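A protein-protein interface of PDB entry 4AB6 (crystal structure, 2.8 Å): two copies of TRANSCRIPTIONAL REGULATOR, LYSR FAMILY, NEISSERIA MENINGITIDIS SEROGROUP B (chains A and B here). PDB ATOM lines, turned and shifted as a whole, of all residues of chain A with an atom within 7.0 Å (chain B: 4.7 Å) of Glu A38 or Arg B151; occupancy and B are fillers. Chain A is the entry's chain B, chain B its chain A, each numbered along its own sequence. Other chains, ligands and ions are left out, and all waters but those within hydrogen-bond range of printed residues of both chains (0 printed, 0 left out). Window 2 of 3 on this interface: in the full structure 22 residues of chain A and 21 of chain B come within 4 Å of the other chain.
Of the 16 printed residues of chain A, 5 touch a printed residue of chain B. Along chain A the printed residues that touch a printed residue of chain B span positions 31 to 41. Of the 9 printed residues of chain B, 4 touch a printed residue of chain A. Hydrophobic or aromatic side chains of chain B within 4 Å of the printed part of chain A: Leu B146. Among the printed residues, 9 pairs touch across the chains. Among the printed residues, Asp or Glu carboxylates within 4 Å of a Lys or Arg side-chain nitrogen of the other chain: Glu A38 with Arg B151 (2.5 Å) and Asp A40 with Arg B135 (2.9 Å).
No position is printed for both chains. Of the 9 pairs that touch across the chains among the printed residues, none has its exchanged pair printed and touching as well.
The side-chain carboxylate (OD1) of Asp A40 lies within salt-bridge range of the guanidinium group (NH2) of Arg B135. NH2 of Arg B135 lies within hydrogen-bond range of O of Ile A41, 2.6 Å away. The guanidinium group (NH2) of Arg B151 is in salt-bridge range of the side-chain carboxylate (OE1) of Glu A38 (2.5 Å). The backbone carbonyl oxygen of Leu A39 sits at hydrogen-bond distance from the guanidinium group of Arg B151 (2.9 Å).
Among the printed residues, pairs that only touch across the chains: Arg A31 with Ser B149 (3.6 Å), Leu A39 with Ser B149 (3.2 Å), Asp A40 with Leu B146 (3.4 Å), Asp A40 with Arg B151 (3.2 Å) and Ile A41 with Leu B146 (3.6 Å).
N of Arg B151 lies within hydrogen-bond range of O of Leu B146 (2.9 Å). O of Ser B149 lies within hydrogen-bond range of NE of Arg B151 (3.4 Å). The backbone carbonyl oxygen (O) of Gly A8 lies within hydrogen-bond range of the backbone NH (N) of Glu A38, 3.1 Å away. The backbone NH (N) of Leu A10 is in hydrogen-bond range of the backbone carbonyl oxygen (O) of Glu A38 (2.8 Å). O of Leu A10 is in hydrogen-bond range of N of Asp A40 (2.9 Å).
Glu A38 touches just one residue of chain B: Arg B151 (2.5 Å). Of the printed residues of chain B, Leu A39 touches Ser B149 and Arg B151. Of the printed residues of chain B, Asp A40 touches Arg B135, Leu B146 and Arg B151. Ile B109 touches none of the printed residues of chain A. Printed residues of chain A within 4 Å of Arg B135: Asp A40 and Ile A41. Of the printed residues of chain A, Leu B146 touches Asp A40 and Ile A41. Printed residues of chain A within 4 Å of Ser B149: Arg A31 (3.6 Å) and Leu A39 (3.2 Å). Arg B151 touches just these residues of chain A: Glu A38, Leu A39 and Asp A40. The nearest printed residue of chain B that does not touch Glu A38 is Ser B149 (4.8 Å). The nearest residue of chain A that does not touch Arg B151 is Ile A41 (5.2 Å). The nearest printed residue of chain B that does not touch Asp A40 is Ser B149 (4.5 Å).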
ATOM      1  N   GLY A   8     -27.014 -30.293  -4.076  1.00  0.00           N
ATOM      2  CA  GLY A   8     -27.797 -29.494  -5.014  1.00  0.00           C
ATOM      3  C   GLY A   8     -27.153 -28.200  -5.495  1.00  0.00           C
ATOM      4  O   GLY A   8     -25.919 -28.096  -5.544  1.00  0.00           O
ATOM      5  N   GLU A   9     -27.983 -27.216  -5.883  1.00  0.00           N
ATOM      6  CA  GLU A   9     -27.502 -25.916  -6.368  1.00  0.00           C
ATOM      7  C   GLU A   9     -28.335 -24.715  -5.913  1.00  0.00           C
ATOM      8  O   GLU A   9     -29.552 -24.830  -5.766  1.00  0.00           O
ATOM      9  CB  GLU A   9     -27.273 -25.911  -7.885  1.00  0.00           C
ATOM     10  CG  GLU A   9     -28.529 -26.005  -8.737  1.00  0.00           C
ATOM     11  CD  GLU A   9     -28.316 -25.786 -10.220  1.00  0.00           C
ATOM     12  OE1 GLU A   9     -27.174 -25.486 -10.635  1.00  0.00           O
ATOM     13  OE2 GLU A   9     -29.307 -25.905 -10.973  1.00  0.00           O
ATOM     14  N   LEU A  10     -27.661 -23.566  -5.694  1.00  0.00           N
ATOM     15  CA  LEU A  10     -28.278 -22.322  -5.245  1.00  0.00           C
ATOM     16  C   LEU A  10     -27.929 -21.142  -6.162  1.00  0.00           C
ATOM     17  O   LEU A  10     -26.893 -20.488  -5.981  1.00  0.00           O
ATOM     18  CB  LEU A  10     -27.874 -22.004  -3.790  1.00  0.00           C
ATOM     19  CG  LEU A  10     -28.965 -21.543  -2.813  1.00  0.00           C
ATOM     20  CD1 LEU A  10     -28.361 -21.171  -1.480  1.00  0.00           C
ATOM     21  CD2 LEU A  10     -29.745 -20.349  -3.335  1.00  0.00           C
ATOM     22  N   ARG A  11     -28.808 -20.862  -7.132  1.00  0.00           N
ATOM     23  CA  ARG A  11     -28.665 -19.739  -8.058  1.00  0.00           C
ATOM     24  C   ARG A  11     -29.559 -18.624  -7.523  1.00  0.00           C
ATOM     25  O   ARG A  11     -30.783 -18.765  -7.523  1.00  0.00           O
ATOM     26  CB  ARG A  11     -29.065 -20.149  -9.486  1.00  0.00           C
ATOM     27  CG  ARG A  11     -28.244 -21.305 -10.070  1.00  0.00           C
ATOM     28  CD  ARG A  11     -28.900 -21.891 -11.303  1.00  0.00           C
ATOM     29  NE  ARG A  11     -30.149 -22.583 -10.982  1.00  0.00           N
ATOM     30  CZ  ARG A  11     -30.997 -23.062 -11.887  1.00  0.00           C
ATOM     31  NH1 ARG A  11     -30.744 -22.927 -13.186  1.00  0.00           N
ATOM     32  NH2 ARG A  11     -32.110 -23.676 -11.500  1.00  0.00           N
ATOM     33  N   PHE A  30     -22.663 -19.202   4.384  1.00  0.00           N
ATOM     34  CA  PHE A  30     -23.302 -20.398   3.832  1.00  0.00           C
ATOM     35  C   PHE A  30     -22.294 -21.428   3.296  1.00  0.00           C
ATOM     36  O   PHE A  30     -22.329 -22.581   3.724  1.00  0.00           O
ATOM     37  CB  PHE A  30     -24.316 -19.994   2.746  1.00  0.00           C
ATOM     38  CG  PHE A  30     -25.079 -21.129   2.099  1.00  0.00           C
ATOM     39  CD1 PHE A  30     -26.282 -21.573   2.633  1.00  0.00           C
ATOM     40  CD2 PHE A  30     -24.617 -21.723   0.928  1.00  0.00           C
ATOM     41  CE1 PHE A  30     -26.992 -22.614   2.031  1.00  0.00           C
ATOM     42  CE2 PHE A  30     -25.322 -22.773   0.328  1.00  0.00           C
ATOM     43  CZ  PHE A  30     -26.503 -23.217   0.889  1.00  0.00           C
ATOM     44  N   ARG A  31     -21.427 -21.016   2.342  1.00  0.00           N
ATOM     45  CA  ARG A  31     -20.425 -21.842   1.652  1.00  0.00           C
ATOM     46  C   ARG A  31     -19.723 -22.935   2.470  1.00  0.00           C
ATOM     47  O   ARG A  31     -19.840 -24.092   2.065  1.00  0.00           O
ATOM     48  CB  ARG A  31     -19.417 -20.993   0.872  1.00  0.00           C
ATOM     49  CG  ARG A  31     -19.583 -21.106  -0.623  1.00  0.00           C
ATOM     50  CD  ARG A  31     -18.331 -20.743  -1.377  1.00  0.00           C
ATOM     51  NE  ARG A  31     -17.413 -21.880  -1.504  1.00  0.00           N
ATOM     52  CZ  ARG A  31     -17.509 -22.844  -2.418  1.00  0.00           C
ATOM     53  NH1 ARG A  31     -18.497 -22.831  -3.309  1.00  0.00           N
ATOM     54  NH2 ARG A  31     -16.620 -23.829  -2.449  1.00  0.00           N
ATOM     55  N   TRP A  34     -22.240 -25.774   3.577  1.00  0.00           N
ATOM     56  CA  TRP A  34     -22.775 -26.576   2.478  1.00  0.00           C
ATOM     57  C   TRP A  34     -21.759 -26.610   1.315  1.00  0.00           C
ATOM     58  O   TRP A  34     -21.942 -25.905   0.317  1.00  0.00           O
ATOM     59  CB  TRP A  34     -24.143 -26.022   2.034  1.00  0.00           C
ATOM     60  CG  TRP A  34     -25.124 -25.846   3.160  1.00  0.00           C
ATOM     61  CD1 TRP A  34     -25.257 -24.754   3.970  1.00  0.00           C
ATOM     62  CD2 TRP A  34     -26.075 -26.810   3.627  1.00  0.00           C
ATOM     63  NE1 TRP A  34     -26.240 -24.972   4.905  1.00  0.00           N
ATOM     64  CE2 TRP A  34     -26.767 -26.223   4.713  1.00  0.00           C
ATOM     65  CE3 TRP A  34     -26.424 -28.111   3.224  1.00  0.00           C
ATOM     66  CZ2 TRP A  34     -27.784 -26.891   5.399  1.00  0.00           C
ATOM     67  CZ3 TRP A  34     -27.439 -28.768   3.901  1.00  0.00           C
ATOM     68  CH2 TRP A  34     -28.103 -28.162   4.978  1.00  0.00           C
ATOM     69  N   PRO A  35     -20.660 -27.397   1.430  1.00  0.00           N
ATOM     70  CA  PRO A  35     -19.655 -27.410   0.354  1.00  0.00           C
ATOM     71  C   PRO A  35     -20.119 -28.060  -0.951  1.00  0.00           C
ATOM     72  O   PRO A  35     -19.519 -27.812  -2.000  1.00  0.00           O
ATOM     73  CB  PRO A  35     -18.479 -28.163   0.979  1.00  0.00           C
ATOM     74  CG  PRO A  35     -19.101 -29.051   1.989  1.00  0.00           C
ATOM     75  CD  PRO A  35     -20.265 -28.285   2.543  1.00  0.00           C
ATOM     76  N   GLN A  36     -21.182 -28.886  -0.879  1.00  0.00           N
ATOM     77  CA  GLN A  36     -21.755 -29.600  -2.027  1.00  0.00           C
ATOM     78  C   GLN A  36     -22.717 -28.744  -2.858  1.00  0.00           C
ATOM     79  O   GLN A  36     -22.878 -29.014  -4.050  1.00  0.00           O
ATOM     80  CB  GLN A  36     -22.446 -30.901  -1.589  1.00  0.00           C
ATOM     81  CG  GLN A  36     -21.545 -31.893  -0.832  1.00  0.00           C
ATOM     82  CD  GLN A  36     -20.355 -32.431  -1.612  1.00  0.00           C
ATOM     83  OE1 GLN A  36     -20.381 -32.579  -2.838  1.00  0.00           O
ATOM     84  NE2 GLN A  36     -19.296 -32.777  -0.894  1.00  0.00           N
ATOM     85  N   VAL A  37     -23.361 -27.731  -2.236  1.00  0.00           N
ATOM     86  CA  VAL A  37     -24.303 -26.823  -2.902  1.00  0.00           C
ATOM     87  C   VAL A  37     -23.536 -25.830  -3.793  1.00  0.00           C
ATOM     88  O   VAL A  37     -22.693 -25.077  -3.300  1.00  0.00           O
ATOM     89  CB  VAL A  37     -25.279 -26.117  -1.915  1.00  0.00           C
ATOM     90  CG1 VAL A  37     -26.252 -25.202  -2.652  1.00  0.00           C
ATOM     91  CG2 VAL A  37     -26.043 -27.131  -1.066  1.00  0.00           C
ATOM     92  N   GLU A  38     -23.834 -25.849  -5.108  1.00  0.00           N
ATOM     93  CA  GLU A  38     -23.204 -24.982  -6.106  1.00  0.00           C
ATOM     94  C   GLU A  38     -23.860 -23.592  -6.094  1.00  0.00           C
ATOM     95  O   GLU A  38     -24.978 -23.437  -6.592  1.00  0.00           O
ATOM     96  CB  GLU A  38     -23.248 -25.616  -7.516  1.00  0.00           C
ATOM     97  CG  GLU A  38     -22.456 -26.904  -7.680  1.00  0.00           C
ATOM     98  CD  GLU A  38     -20.955 -26.796  -7.917  1.00  0.00           C
ATOM     99  OE1 GLU A  38     -20.496 -25.836  -8.585  1.00  0.00           O
ATOM    100  OE2 GLU A  38     -20.242 -27.735  -7.491  1.00  0.00           O
ATOM    101  N   LEU A  39     -23.179 -22.593  -5.498  1.00  0.00           N
ATOM    102  CA  LEU A  39     -23.683 -21.221  -5.406  1.00  0.00           C
ATOM    103  C   LEU A  39     -23.489 -20.418  -6.702  1.00  0.00           C
ATOM    104  O   LEU A  39     -22.527 -20.653  -7.434  1.00  0.00           O
ATOM    105  CB  LEU A  39     -23.037 -20.477  -4.224  1.00  0.00           C
ATOM    106  CG  LEU A  39     -23.682 -20.595  -2.855  1.00  0.00           C
ATOM    107  CD1 LEU A  39     -22.792 -20.001  -1.804  1.00  0.00           C
ATOM    108  CD2 LEU A  39     -24.995 -19.847  -2.803  1.00  0.00           C
ATOM    109  N   ASP A  40     -24.399 -19.460  -6.968  1.00  0.00           N
ATOM    110  CA  ASP A  40     -24.383 -18.568  -8.138  1.00  0.00           C
ATOM    111  C   ASP A  40     -25.337 -17.377  -7.963  1.00  0.00           C
ATOM    112  O   ASP A  40     -26.302 -17.478  -7.209  1.00  0.00           O
ATOM    113  CB  ASP A  40     -24.780 -19.342  -9.417  1.00  0.00           C
ATOM    114  CG  ASP A  40     -24.429 -18.672 -10.741  1.00  0.00           C
ATOM    115  OD1 ASP A  40     -23.653 -17.688 -10.728  1.00  0.00           O
ATOM    116  OD2 ASP A  40     -24.872 -19.172 -11.790  1.00  0.00           O
ATOM    117  N   ILE A  41     -25.061 -16.252  -8.659  1.00  0.00           N
ATOM    118  CA  ILE A  41     -25.910 -15.049  -8.686  1.00  0.00           C
ATOM    119  C   ILE A  41     -26.403 -14.900 -10.133  1.00  0.00           C
ATOM    120  O   ILE A  41     -25.588 -14.949 -11.055  1.00  0.00           O
ATOM    121  CB  ILE A  41     -25.195 -13.758  -8.191  1.00  0.00           C
ATOM    122  CG1 ILE A  41     -24.468 -13.980  -6.852  1.00  0.00           C
ATOM    123  CG2 ILE A  41     -26.180 -12.580  -8.084  1.00  0.00           C
ATOM    124  CD1 ILE A  41     -23.163 -13.353  -6.794  1.00  0.00           C
ATOM    125  N   ASP A  59     -32.882 -20.481  -8.209  1.00  0.00           N
ATOM    126  CA  ASP A  59     -33.353 -21.405  -7.174  1.00  0.00           C
ATOM    127  C   ASP A  59     -33.892 -20.682  -5.941  1.00  0.00           C
ATOM    128  O   ASP A  59     -34.681 -21.256  -5.189  1.00  0.00           O
ATOM    129  CB  ASP A  59     -32.259 -22.423  -6.818  1.00  0.00           C
ATOM    130  CG  ASP A  59     -31.723 -23.165  -8.033  1.00  0.00           C
ATOM    131  OD1 ASP A  59     -32.537 -23.748  -8.782  1.00  0.00           O
ATOM    132  OD2 ASP A  59     -30.501 -23.112  -8.266  1.00  0.00           O
ATOM    133  N   TYR A 197     -30.962 -26.721   2.892  1.00  0.00           N
ATOM    134  CA  TYR A 197     -30.027 -25.621   2.624  1.00  0.00           C
ATOM    135  C   TYR A 197     -30.680 -24.289   2.256  1.00  0.00           C
ATOM    136  O   TYR A 197     -30.150 -23.241   2.625  1.00  0.00           O
ATOM    137  CB  TYR A 197     -28.916 -26.009   1.634  1.00  0.00           C
ATOM    138  CG  TYR A 197     -29.383 -26.389   0.250  1.00  0.00           C
ATOM    139  CD1 TYR A 197     -29.484 -25.435  -0.758  1.00  0.00           C
ATOM    140  CD2 TYR A 197     -29.635 -27.717  -0.079  1.00  0.00           C
ATOM    141  CE1 TYR A 197     -29.892 -25.783  -2.045  1.00  0.00           C
ATOM    142  CE2 TYR A 197     -30.038 -28.079  -1.365  1.00  0.00           C
ATOM    143  CZ  TYR A 197     -30.168 -27.108  -2.344  1.00  0.00           C
ATOM    144  OH  TYR A 197     -30.572 -27.456  -3.610  1.00  0.00           O
ATOM    145  N   THR B 107     -13.868 -19.167 -16.555  1.00  0.00           N
ATOM    146  CA  THR B 107     -14.818 -18.086 -16.812  1.00  0.00           C
ATOM    147  C   THR B 107     -14.207 -16.813 -16.224  1.00  0.00           C
ATOM    148  O   THR B 107     -13.822 -16.798 -15.054  1.00  0.00           O
ATOM    149  CB  THR B 107     -16.203 -18.426 -16.235  1.00  0.00           C
ATOM    150  OG1 THR B 107     -16.721 -19.555 -16.928  1.00  0.00           O
ATOM    151  CG2 THR B 107     -17.194 -17.277 -16.358  1.00  0.00           C
ATOM    152  N   ILE B 109     -14.605 -13.195 -14.823  1.00  0.00           N
ATOM    153  CA  ILE B 109     -15.563 -12.265 -14.223  1.00  0.00           C
ATOM    154  C   ILE B 109     -14.960 -10.854 -14.197  1.00  0.00           C
ATOM    155  O   ILE B 109     -13.955 -10.613 -13.526  1.00  0.00           O
ATOM    156  CB  ILE B 109     -16.075 -12.735 -12.831  1.00  0.00           C
ATOM    157  CG1 ILE B 109     -16.565 -14.204 -12.891  1.00  0.00           C
ATOM    158  CG2 ILE B 109     -17.189 -11.799 -12.318  1.00  0.00           C
ATOM    159  CD1 ILE B 109     -16.577 -14.917 -11.600  1.00  0.00           C
ATOM    160  N   ARG B 135     -18.129 -13.000 -17.878  1.00  0.00           N
ATOM    161  CA  ARG B 135     -19.209 -12.897 -16.910  1.00  0.00           C
ATOM    162  C   ARG B 135     -19.164 -11.458 -16.405  1.00  0.00           C
ATOM    163  O   ARG B 135     -18.103 -10.985 -15.984  1.00  0.00           O
ATOM    164  CB  ARG B 135     -19.021 -13.906 -15.768  1.00  0.00           C
ATOM    165  CG  ARG B 135     -20.213 -14.013 -14.823  1.00  0.00           C
ATOM    166  CD  ARG B 135     -21.077 -15.217 -15.141  1.00  0.00           C
ATOM    167  NE  ARG B 135     -22.364 -15.133 -14.455  1.00  0.00           N
ATOM    168  CZ  ARG B 135     -22.738 -15.892 -13.432  1.00  0.00           C
ATOM    169  NH1 ARG B 135     -21.931 -16.842 -12.972  1.00  0.00           N
ATOM    170  NH2 ARG B 135     -23.932 -15.732 -12.881  1.00  0.00           N
ATOM    171  N   LEU B 146     -19.099 -14.392  -6.559  1.00  0.00           N
ATOM    172  CA  LEU B 146     -19.174 -15.230  -7.754  1.00  0.00           C
ATOM    173  C   LEU B 146     -17.902 -16.080  -7.824  1.00  0.00           C
ATOM    174  O   LEU B 146     -17.984 -17.287  -8.049  1.00  0.00           O
ATOM    175  CB  LEU B 146     -19.336 -14.388  -9.027  1.00  0.00           C
ATOM    176  CG  LEU B 146     -20.749 -13.915  -9.379  1.00  0.00           C
ATOM    177  CD1 LEU B 146     -20.712 -12.878 -10.482  1.00  0.00           C
ATOM    178  CD2 LEU B 146     -21.662 -15.079  -9.794  1.00  0.00           C
ATOM    179  N   VAL B 147     -16.738 -15.450  -7.556  1.00  0.00           N
ATOM    180  CA  VAL B 147     -15.421 -16.087  -7.537  1.00  0.00           C
ATOM    181  C   VAL B 147     -15.354 -17.136  -6.409  1.00  0.00           C
ATOM    182  O   VAL B 147     -14.980 -18.282  -6.672  1.00  0.00           O
ATOM    183  CB  VAL B 147     -14.283 -15.031  -7.466  1.00  0.00           C
ATOM    184  CG1 VAL B 147     -12.931 -15.685  -7.262  1.00  0.00           C
ATOM    185  CG2 VAL B 147     -14.260 -14.157  -8.719  1.00  0.00           C
ATOM    186  N   SER B 149     -17.779 -18.723  -4.962  1.00  0.00           N
ATOM    187  CA  SER B 149     -18.734 -19.796  -5.255  1.00  0.00           C
ATOM    188  C   SER B 149     -18.317 -20.678  -6.451  1.00  0.00           C
ATOM    189  O   SER B 149     -19.105 -21.512  -6.914  1.00  0.00           O
ATOM    190  CB  SER B 149     -20.120 -19.205  -5.489  1.00  0.00           C
ATOM    191  OG  SER B 149     -20.530 -18.432  -4.369  1.00  0.00           O
ATOM    192  N   ARG B 150     -17.060 -20.504  -6.922  1.00  0.00           N
ATOM    193  CA  ARG B 150     -16.448 -21.210  -8.053  1.00  0.00           C
ATOM    194  C   ARG B 150     -17.182 -20.995  -9.395  1.00  0.00           C
ATOM    195  O   ARG B 150     -17.279 -21.913 -10.214  1.00  0.00           O
ATOM    196  CB  ARG B 150     -16.208 -22.700  -7.736  1.00  0.00           C
ATOM    197  CG  ARG B 150     -15.141 -22.950  -6.676  1.00  0.00           C
ATOM    198  CD  ARG B 150     -14.743 -24.405  -6.507  1.00  0.00           C
ATOM    199  NE  ARG B 150     -14.677 -25.156  -7.761  1.00  0.00           N
ATOM    200  CZ  ARG B 150     -14.808 -26.483  -7.852  1.00  0.00           C
ATOM    201  NH1 ARG B 150     -15.013 -27.215  -6.760  1.00  0.00           N
ATOM    202  NH2 ARG B 150     -14.746 -27.084  -9.033  1.00  0.00           N
ATOM    203  N   ARG B 151     -17.674 -19.761  -9.624  1.00  0.00           N
ATOM    204  CA  ARG B 151     -18.360 -19.385 -10.864  1.00  0.00           C
ATOM    205  C   ARG B 151     -17.368 -18.877 -11.904  1.00  0.00           C
ATOM    206  O   ARG B 151     -17.721 -18.704 -13.072  1.00  0.00           O
ATOM    207  CB  ARG B 151     -19.477 -18.351 -10.612  1.00  0.00           C
ATOM    208  CG  ARG B 151     -20.601 -18.818  -9.687  1.00  0.00           C
ATOM    209  CD  ARG B 151     -21.399 -19.966 -10.273  1.00  0.00           C
ATOM    210  NE  ARG B 151     -20.888 -21.251  -9.812  1.00  0.00           N
ATOM    211  CZ  ARG B 151     -21.507 -22.414  -9.977  1.00  0.00           C
ATOM    212  NH1 ARG B 151     -22.685 -22.468 -10.581  1.00  0.00           N
ATOM    213  NH2 ARG B 151     -20.954 -23.535  -9.530  1.00  0.00           N
ATOM    214  N   GLY B 152     -16.136 -18.662 -11.462  1.00  0.00           N
ATOM    215  CA  GLY B 152     -15.053 -18.193 -12.307  1.00  0.00           C
ATOM    216  C   GLY B 152     -13.961 -17.503 -11.520  1.00  0.00           C
ATOM    217  O   GLY B 152     -13.980 -17.496 -10.288  1.00  0.00           O
